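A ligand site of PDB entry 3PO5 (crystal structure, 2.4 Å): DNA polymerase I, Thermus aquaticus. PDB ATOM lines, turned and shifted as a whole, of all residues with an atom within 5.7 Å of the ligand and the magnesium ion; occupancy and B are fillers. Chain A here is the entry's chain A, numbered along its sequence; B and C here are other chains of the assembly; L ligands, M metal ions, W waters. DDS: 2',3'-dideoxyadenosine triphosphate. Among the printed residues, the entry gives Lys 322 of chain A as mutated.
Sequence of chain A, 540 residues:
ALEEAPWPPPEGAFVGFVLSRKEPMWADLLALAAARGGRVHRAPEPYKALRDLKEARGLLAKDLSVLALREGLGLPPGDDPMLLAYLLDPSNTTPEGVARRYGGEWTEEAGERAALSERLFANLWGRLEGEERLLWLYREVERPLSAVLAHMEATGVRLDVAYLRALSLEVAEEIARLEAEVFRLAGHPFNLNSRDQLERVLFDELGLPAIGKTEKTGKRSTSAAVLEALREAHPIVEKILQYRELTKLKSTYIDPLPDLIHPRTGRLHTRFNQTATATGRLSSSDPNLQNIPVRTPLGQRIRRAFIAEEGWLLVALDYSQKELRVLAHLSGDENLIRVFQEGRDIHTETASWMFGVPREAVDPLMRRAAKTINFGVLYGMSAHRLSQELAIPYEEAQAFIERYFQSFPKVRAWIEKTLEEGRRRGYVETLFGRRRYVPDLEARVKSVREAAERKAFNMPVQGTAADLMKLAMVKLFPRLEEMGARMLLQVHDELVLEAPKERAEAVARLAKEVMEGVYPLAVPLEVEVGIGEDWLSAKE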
ATOM      1  N   ARG A 295      21.776  -3.207 -15.568  1.00  0.00           N
ATOM      2  CA  ARG A 295      23.000  -3.320 -14.767  1.00  0.00           C
ATOM      3  C   ARG A 295      23.102  -4.638 -14.018  1.00  0.00           C
ATOM      4  O   ARG A 295      24.159  -4.979 -13.494  1.00  0.00           O
ATOM      5  CB  ARG A 295      23.096  -2.152 -13.778  1.00  0.00           C
ATOM      6  CG  ARG A 295      23.056  -0.770 -14.440  1.00  0.00           C
ATOM      7  CD  ARG A 295      23.020   0.366 -13.416  1.00  0.00           C
ATOM      8  NE  ARG A 295      22.900   1.674 -14.056  1.00  0.00           N
ATOM      9  CZ  ARG A 295      22.796   2.834 -13.403  1.00  0.00           C
ATOM     10  NH1 ARG A 295      22.803   2.858 -12.083  1.00  0.00           N
ATOM     11  NH2 ARG A 295      22.696   3.974 -14.078  1.00  0.00           N
ATOM     12  N   ASP A 318      25.549   4.909 -28.571  1.00  0.00           N
ATOM     13  CA  ASP A 318      25.801   5.159 -27.176  1.00  0.00           C
ATOM     14  C   ASP A 318      27.016   6.064 -27.017  1.00  0.00           C
ATOM     15  O   ASP A 318      28.142   5.600 -27.138  1.00  0.00           O
ATOM     16  CB  ASP A 318      26.026   3.800 -26.502  1.00  0.00           C
ATOM     17  CG  ASP A 318      26.059   3.869 -24.999  1.00  0.00           C
ATOM     18  OD1 ASP A 318      26.778   4.735 -24.445  1.00  0.00           O
ATOM     19  OD2 ASP A 318      25.358   3.035 -24.363  1.00  0.00           O
ATOM     20  N   TYR A 319      26.793   7.354 -26.763  1.00  0.00           N
ATOM     21  CA  TYR A 319      27.906   8.267 -26.496  1.00  0.00           C
ATOM     22  C   TYR A 319      28.706   7.810 -25.286  1.00  0.00           C
ATOM     23  O   TYR A 319      28.130   7.455 -24.250  1.00  0.00           O
ATOM     24  CB  TYR A 319      27.399   9.680 -26.217  1.00  0.00           C
ATOM     25  CG  TYR A 319      26.913  10.496 -27.396  1.00  0.00           C
ATOM     26  CD1 TYR A 319      27.816  11.072 -28.285  1.00  0.00           C
ATOM     27  CD2 TYR A 319      25.552  10.745 -27.581  1.00  0.00           C
ATOM     28  CE1 TYR A 319      27.377  11.851 -29.347  1.00  0.00           C
ATOM     29  CE2 TYR A 319      25.108  11.510 -28.643  1.00  0.00           C
ATOM     30  CZ  TYR A 319      26.027  12.072 -29.521  1.00  0.00           C
ATOM     31  OH  TYR A 319      25.588  12.841 -30.552  1.00  0.00           O
ATOM     32  N   SER A 320      30.028   7.831 -25.382  1.00  0.00           N
ATOM     33  CA  SER A 320      30.889   7.436 -24.276  1.00  0.00           C
ATOM     34  C   SER A 320      31.260   8.633 -23.417  1.00  0.00           C
ATOM     35  O   SER A 320      31.642   9.678 -23.943  1.00  0.00           O
ATOM     36  CB  SER A 320      32.162   6.780 -24.800  1.00  0.00           C
ATOM     37  OG  SER A 320      31.860   5.637 -25.592  1.00  0.00           O
ATOM     38  N   GLN A 321      31.169   8.476 -22.095  1.00  0.00           N
ATOM     39  CA  GLN A 321      31.486   9.547 -21.159  1.00  0.00           C
ATOM     40  C   GLN A 321      30.943  10.885 -21.649  1.00  0.00           C
ATOM     41  O   GLN A 321      31.647  11.903 -21.633  1.00  0.00           O
ATOM     42  CB  GLN A 321      32.997   9.656 -20.942  1.00  0.00           C
ATOM     43  CG  GLN A 321      33.679   8.358 -20.578  1.00  0.00           C
ATOM     44  CD  GLN A 321      34.115   7.569 -21.803  1.00  0.00           C
ATOM     45  OE1 GLN A 321      34.573   8.139 -22.785  1.00  0.00           O
ATOM     46  NE2 GLN A 321      33.965   6.253 -21.738  1.00  0.00           N
ATOM     47  N   LYS A 322      29.689  10.890 -22.069  1.00  0.00           N
ATOM     48  CA  LYS A 322      29.096  12.069 -22.672  1.00  0.00           C
ATOM     49  C   LYS A 322      29.232  13.331 -21.811  1.00  0.00           C
ATOM     50  O   LYS A 322      29.779  14.330 -22.277  1.00  0.00           O
ATOM     51  CB  LYS A 322      27.613  11.836 -22.975  1.00  0.00           C
ATOM     52  CG  LYS A 322      26.941  13.033 -23.628  1.00  0.00           C
ATOM     53  CD  LYS A 322      27.673  13.469 -24.898  1.00  0.00           C
ATOM     54  CE  LYS A 322      26.882  14.512 -25.664  1.00  0.00           C
ATOM     55  NZ  LYS A 322      25.509  14.012 -25.938  1.00  0.00           N
ATOM     56  N   GLU A 323      28.734  13.282 -20.580  1.00  0.00           N
ATOM     57  CA  GLU A 323      28.688  14.498 -19.770  1.00  0.00           C
ATOM     58  C   GLU A 323      30.081  14.931 -19.321  1.00  0.00           C
ATOM     59  O   GLU A 323      30.333  16.121 -19.139  1.00  0.00           O
ATOM     60  CB  GLU A 323      27.718  14.314 -18.592  1.00  0.00           C
ATOM     61  CG  GLU A 323      26.275  14.131 -19.052  1.00  0.00           C
ATOM     62  CD  GLU A 323      25.258  14.228 -17.925  1.00  0.00           C
ATOM     63  OE1 GLU A 323      24.122  13.735 -18.101  1.00  0.00           O
ATOM     64  OE2 GLU A 323      25.589  14.793 -16.858  1.00  0.00           O
ATOM     65  N   HIS A 347      38.129   6.256 -17.409  1.00  0.00           N
ATOM     66  CA  HIS A 347      38.024   5.661 -16.072  1.00  0.00           C
ATOM     67  C   HIS A 347      39.178   4.701 -15.839  1.00  0.00           C
ATOM     68  O   HIS A 347      39.035   3.690 -15.134  1.00  0.00           O
ATOM     69  CB  HIS A 347      36.683   4.951 -15.937  1.00  0.00           C
ATOM     70  CG  HIS A 347      35.513   5.822 -16.271  1.00  0.00           C
ATOM     71  ND1 HIS A 347      34.247   5.315 -16.502  1.00  0.00           N
ATOM     72  CD2 HIS A 347      35.423   7.163 -16.424  1.00  0.00           C
ATOM     73  CE1 HIS A 347      33.431   6.314 -16.777  1.00  0.00           C
ATOM     74  NE2 HIS A 347      34.117   7.446 -16.745  1.00  0.00           N
ATOM     75  N   LYS A 371      36.038   6.147 -11.823  1.00  0.00           N
ATOM     76  CA  LYS A 371      34.725   6.223 -12.463  1.00  0.00           C
ATOM     77  C   LYS A 371      33.668   6.800 -11.530  1.00  0.00           C
ATOM     78  O   LYS A 371      33.093   7.846 -11.797  1.00  0.00           O
ATOM     79  CB  LYS A 371      34.275   4.855 -12.946  1.00  0.00           C
ATOM     80  CG  LYS A 371      32.847   4.845 -13.508  1.00  0.00           C
ATOM     81  CD  LYS A 371      32.260   3.450 -13.534  1.00  0.00           C
ATOM     82  CE  LYS A 371      32.075   2.944 -14.957  1.00  0.00           C
ATOM     83  NZ  LYS A 371      30.634   2.941 -15.329  1.00  0.00           N
ATOM     84  N   PHE A 375      31.659  10.412 -12.059  1.00  0.00           N
ATOM     85  CA  PHE A 375      30.217  10.587 -12.021  1.00  0.00           C
ATOM     86  C   PHE A 375      29.845  11.536 -10.903  1.00  0.00           C
ATOM     87  O   PHE A 375      28.969  12.388 -11.061  1.00  0.00           O
ATOM     88  CB  PHE A 375      29.513   9.247 -11.790  1.00  0.00           C
ATOM     89  CG  PHE A 375      29.590   8.282 -12.943  1.00  0.00           C
ATOM     90  CD1 PHE A 375      30.111   8.688 -14.167  1.00  0.00           C
ATOM     91  CD2 PHE A 375      29.142   6.978 -12.803  1.00  0.00           C
ATOM     92  CE1 PHE A 375      30.182   7.791 -15.232  1.00  0.00           C
ATOM     93  CE2 PHE A 375      29.217   6.094 -13.857  1.00  0.00           C
ATOM     94  CZ  PHE A 375      29.741   6.491 -15.071  1.00  0.00           C
ATOM     95  N   LEU A 378      29.915  15.616 -11.305  1.00  0.00           N
ATOM     96  CA  LEU A 378      28.757  16.210 -11.965  1.00  0.00           C
ATOM     97  C   LEU A 378      27.629  16.502 -10.976  1.00  0.00           C
ATOM     98  O   LEU A 378      26.908  17.473 -11.117  1.00  0.00           O
ATOM     99  CB  LEU A 378      28.222  15.247 -13.020  1.00  0.00           C
ATOM    100  CG  LEU A 378      29.015  15.078 -14.313  1.00  0.00           C
ATOM    101  CD1 LEU A 378      30.502  15.051 -14.046  1.00  0.00           C
ATOM    102  CD2 LEU A 378      28.575  13.798 -15.018  1.00  0.00           C
ATOM    103  N   TYR A 379      27.491  15.632  -9.970  1.00  0.00           N
ATOM    104  CA  TYR A 379      26.386  15.725  -9.015  1.00  0.00           C
ATOM    105  C   TYR A 379      26.794  16.497  -7.761  1.00  0.00           C
ATOM    106  O   TYR A 379      25.944  16.880  -6.971  1.00  0.00           O
ATOM    107  CB  TYR A 379      25.916  14.330  -8.624  1.00  0.00           C
ATOM    108  CG  TYR A 379      25.631  13.430  -9.811  1.00  0.00           C
ATOM    109  CD1 TYR A 379      25.077  13.937 -10.972  1.00  0.00           C
ATOM    110  CD2 TYR A 379      25.946  12.077  -9.771  1.00  0.00           C
ATOM    111  CE1 TYR A 379      24.824  13.120 -12.076  1.00  0.00           C
ATOM    112  CE2 TYR A 379      25.695  11.251 -10.855  1.00  0.00           C
ATOM    113  CZ  TYR A 379      25.133  11.777 -12.017  1.00  0.00           C
ATOM    114  OH  TYR A 379      24.878  10.960 -13.101  1.00  0.00           O
ATOM    115  N   GLU A 389      29.949   4.478  -0.470  1.00  0.00           N
ATOM    116  CA  GLU A 389      29.515   3.753  -1.667  1.00  0.00           C
ATOM    117  C   GLU A 389      30.712   3.150  -2.392  1.00  0.00           C
ATOM    118  O   GLU A 389      30.562   2.510  -3.426  1.00  0.00           O
ATOM    119  CB  GLU A 389      28.740   4.672  -2.600  1.00  0.00           C
ATOM    120  CG  GLU A 389      27.928   3.930  -3.660  1.00  0.00           C
ATOM    121  CD  GLU A 389      28.266   4.379  -5.068  1.00  0.00           C
ATOM    122  OE1 GLU A 389      28.361   5.608  -5.289  1.00  0.00           O
ATOM    123  OE2 GLU A 389      28.423   3.518  -5.962  1.00  0.00           O
ATOM    124  N   ASP A 493      21.718   9.541 -23.361  1.00  0.00           N
ATOM    125  CA  ASP A 493      22.955   9.526 -24.131  1.00  0.00           C
ATOM    126  C   ASP A 493      23.016   8.348 -25.111  1.00  0.00           C
ATOM    127  O   ASP A 493      24.074   8.016 -25.615  1.00  0.00           O
ATOM    128  CB  ASP A 493      24.189   9.513 -23.199  1.00  0.00           C
ATOM    129  CG  ASP A 493      24.306   8.216 -22.378  1.00  0.00           C
ATOM    130  OD1 ASP A 493      23.514   7.278 -22.587  1.00  0.00           O
ATOM    131  OD2 ASP A 493      25.199   8.145 -21.506  1.00  0.00           O
ATOM    132  N   GLU A 528      29.817   4.418 -29.287  1.00  0.00           N
ATOM    133  CA  GLU A 528      29.831   2.981 -29.463  1.00  0.00           C
ATOM    134  C   GLU A 528      28.546   2.565 -30.162  1.00  0.00           C
ATOM    135  O   GLU A 528      27.494   3.133 -29.913  1.00  0.00           O
ATOM    136  CB  GLU A 528      29.944   2.259 -28.129  1.00  0.00           C
ATOM    137  CG  GLU A 528      31.298   2.373 -27.497  1.00  0.00           C
ATOM    138  CD  GLU A 528      31.249   2.148 -25.999  1.00  0.00           C
ATOM    139  OE1 GLU A 528      30.234   1.584 -25.525  1.00  0.00           O
ATOM    140  OE2 GLU A 528      32.199   2.555 -25.299  1.00  0.00           O
ATOM    141  P   2DA B  12      21.906   3.028 -17.711  1.00  0.00           P
ATOM    142  OP1 2DA B  12      21.987   2.303 -19.029  1.00  0.00           O
ATOM    143  OP2 2DA B  12      22.971   2.789 -16.675  1.00  0.00           O
ATOM    144  O5' 2DA B  12      21.879   4.600 -18.043  1.00  0.00           O
ATOM    145  C5' 2DA B  12      21.187   5.050 -19.210  1.00  0.00           C
ATOM    146  C4' 2DA B  12      21.270   6.563 -19.316  1.00  0.00           C
ATOM    147  O4' 2DA B  12      20.413   7.204 -18.360  1.00  0.00           O
ATOM    148  C3' 2DA B  12      22.678   7.034 -19.046  1.00  0.00           C
ATOM    149  C2' 2DA B  12      22.459   8.395 -18.410  1.00  0.00           C
ATOM    150  C1' 2DA B  12      21.095   8.297 -17.744  1.00  0.00           C
ATOM    151  N9  2DA B  12      21.322   7.998 -16.292  1.00  0.00           N
ATOM    152  C8  2DA B  12      21.661   6.796 -15.769  1.00  0.00           C
ATOM    153  N7  2DA B  12      21.795   6.874 -14.425  1.00  0.00           N
ATOM    154  C5  2DA B  12      21.527   8.142 -14.075  1.00  0.00           C
ATOM    155  C6  2DA B  12      21.481   8.900 -12.804  1.00  0.00           C
ATOM    156  N6  2DA B  12      21.750   8.287 -11.624  1.00  0.00           N
ATOM    157  N1  2DA B  12      21.156  10.204 -12.864  1.00  0.00           N
ATOM    158  C2  2DA B  12      20.882  10.827 -14.035  1.00  0.00           C
ATOM    159  N3  2DA B  12      20.909  10.196 -15.229  1.00  0.00           N
ATOM    160  C4  2DA B  12      21.213   8.874 -15.302  1.00  0.00           C
ATOM    161  P    DT C   2      21.796  16.204  -5.456  1.00  0.00           P
ATOM    162  OP1  DT C   2      21.775  17.520  -4.766  1.00  0.00           O
ATOM    163  OP2  DT C   2      20.820  15.162  -5.091  1.00  0.00           O
ATOM    164  O5'  DT C   2      21.688  16.512  -7.025  1.00  0.00           O
ATOM    165  C5'  DT C   2      22.357  17.595  -7.639  1.00  0.00           C
ATOM    166  C4'  DT C   2      22.130  17.521  -9.145  1.00  0.00           C
ATOM    167  O4'  DT C   2      22.898  16.406  -9.660  1.00  0.00           O
ATOM    168  C3'  DT C   2      20.704  17.207  -9.550  1.00  0.00           C
ATOM    169  O3'  DT C   2      19.955  18.377  -9.799  1.00  0.00           O
ATOM    170  C2'  DT C   2      20.855  16.468 -10.859  1.00  0.00           C
ATOM    171  C1'  DT C   2      22.189  15.773 -10.700  1.00  0.00           C
ATOM    172  N1   DT C   2      22.047  14.324 -10.400  1.00  0.00           N
ATOM    173  C2   DT C   2      21.705  13.496 -11.444  1.00  0.00           C
ATOM    174  O2   DT C   2      21.507  13.903 -12.582  1.00  0.00           O
ATOM    175  N3   DT C   2      21.607  12.187 -11.101  1.00  0.00           N
ATOM    176  C4   DT C   2      21.806  11.624  -9.870  1.00  0.00           C
ATOM    177  O4   DT C   2      21.683  10.415  -9.673  1.00  0.00           O
ATOM    178  C5   DT C   2      22.166  12.536  -8.816  1.00  0.00           C
ATOM    179  C7   DT C   2      22.395  12.017  -7.430  1.00  0.00           C
ATOM    180  C6   DT C   2      22.264  13.836  -9.128  1.00  0.00           C
HETATM  181  N1  DDS L   1      25.468   6.790 -10.636  1.00  0.00           N
HETATM  182  C2  DDS L   1      25.244   8.021 -11.136  1.00  0.00           C
HETATM  183  N3  DDS L   1      25.227   8.252 -12.451  1.00  0.00           N
HETATM  184  C4  DDS L   1      25.419   7.254 -13.338  1.00  0.00           C
HETATM  185  C5  DDS L   1      25.650   5.961 -12.856  1.00  0.00           C
HETATM  186  C6  DDS L   1      25.673   5.747 -11.470  1.00  0.00           C
HETATM  187  N6  DDS L   1      25.905   4.436 -10.937  1.00  0.00           N
HETATM  188  N7  DDS L   1      25.822   5.160 -13.920  1.00  0.00           N
HETATM  189  C8  DDS L   1      25.694   5.912 -15.036  1.00  0.00           C
HETATM  190  N9  DDS L   1      25.455   7.191 -14.692  1.00  0.00           N
HETATM  191  PA  DDS L   1      28.070   4.578 -18.298  1.00  0.00           P
HETATM  192  PB  DDS L   1      30.496   5.774 -19.038  1.00  0.00           P
HETATM  193  PG  DDS L   1      31.786   3.331 -19.127  1.00  0.00           P
HETATM  194  C1' DDS L   1      25.265   8.307 -15.650  1.00  0.00           C
HETATM  195  O1A DDS L   1      27.614   3.809 -17.070  1.00  0.00           O
HETATM  196  O1B DDS L   1      30.814   7.172 -18.571  1.00  0.00           O
HETATM  197  O1G DDS L   1      30.958   2.725 -18.016  1.00  0.00           O
HETATM  198  C2' DDS L   1      26.436   9.226 -15.829  1.00  0.00           C
HETATM  199  O2A DDS L   1      28.120   3.664 -19.495  1.00  0.00           O
HETATM  200  O2B DDS L   1      29.950   5.758 -20.452  1.00  0.00           O
HETATM  201  O2G DDS L   1      33.198   2.833 -18.942  1.00  0.00           O
HETATM  202  C3' DDS L   1      26.861   9.104 -17.227  1.00  0.00           C
HETATM  203  O3A DDS L   1      29.466   5.212 -17.952  1.00  0.00           O
HETATM  204  O3B DDS L   1      31.810   4.905 -18.929  1.00  0.00           O
HETATM  205  O3G DDS L   1      31.234   2.949 -20.465  1.00  0.00           O
HETATM  206  C4' DDS L   1      26.163   7.923 -17.753  1.00  0.00           C
HETATM  207  O4' DDS L   1      24.964   7.775 -16.905  1.00  0.00           O
HETATM  208  C5' DDS L   1      26.974   6.776 -17.557  1.00  0.00           C
HETATM  209  O5' DDS L   1      27.067   5.775 -18.527  1.00  0.00           O
HETATM  210 MG    MG M   1      28.904   4.404 -22.094  1.00  0.00          MG
HETATM  211  O   HOH W   1      35.072   1.473 -17.791  1.00  0.00           O
HETATM  212  O   HOH W   2      29.497   4.050 -24.123  1.00  0.00           O
HETATM  213  O   HOH W   3      25.733   5.485 -21.127  1.00  0.00           O
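An oxygen (O1G) of the ligand is in salt-bridge range of the side-chain amino group (NZ) of Lys 371 (2.7 Å).
A nitrogen (N3) of the ligand lies within hydrogen-bond range of the side-chain hydroxyl of Tyr 379 (2.8 Å).
A ring nitrogen (ND1) of His 347 lies close to an oxygen (O3B) of the ligand (3.5 Å).
NH2 of Arg 295 is in hydrogen-bond range of N7 of the ligand (3.3 Å).
The backbone NH (N) of Gln 321 lies close to an oxygen (O2B) of the ligand (3.4 Å).
OP2 of 2DA 12 of chain B is in salt-bridge range of the guanidinium group of Arg 295, 2.8 Å away.
N1 of 2DA 12 of chain B sits close to N3 of DT 2 of chain C, at 2.7 Å.
The backbone NH (N) of Asp 318 is in hydrogen-bond range of the backbone carbonyl oxygen (O) of Glu 528.
The backbone NH of Tyr 319 lies within hydrogen-bond range of the backbone carbonyl oxygen of Asp 493, at 3.0 Å.
Merely in contact with the ligand: Phe 375 (3.2 Å), Asp 493 (3.9 Å) and 2DA 12 of chain B (3.0 Å).
Hydrophobic or aromatic side chains that line the ligand: His 347, Phe 375 and Tyr 379.
Eight residues have an atom within 4 Å of the ligand: Arg 295, Gln 321, His 347, Lys 371, Phe 375, Tyr 379, Asp 493 and 2DA 12 of chain B.
The nearest printed residue that does not touch the ligand is Ser 320 (4.3 Å).
Residues that only touch the magnesium ion: Asp 318 (3.2 Å) and Tyr 319 (3.8 Å).
Of the 17 residues printed, 2 come within 4 Å of the magnesium ion.
Water W2 is bound to the magnesium ion, at 2.1 Å.
The magnesium ion is bound by an oxygen (O2B) of the ligand (2.4 Å).
Slightly farther from the magnesium ion lies O2A of the ligand (2.8 Å).
Water W2 lies within hydrogen-bond range of the side-chain carboxylate of Asp 318 (2.8 Å), the side-chain carboxylate of Glu 528 (2.9 Å) and the side-chain hydroxyl of Ser 320 (3.2 Å).
Water W3 bridges the side-chain carboxylate (OD2) of Asp 493 (2.7 Å) and an oxygen (O5') of the ligand (2.9 Å).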
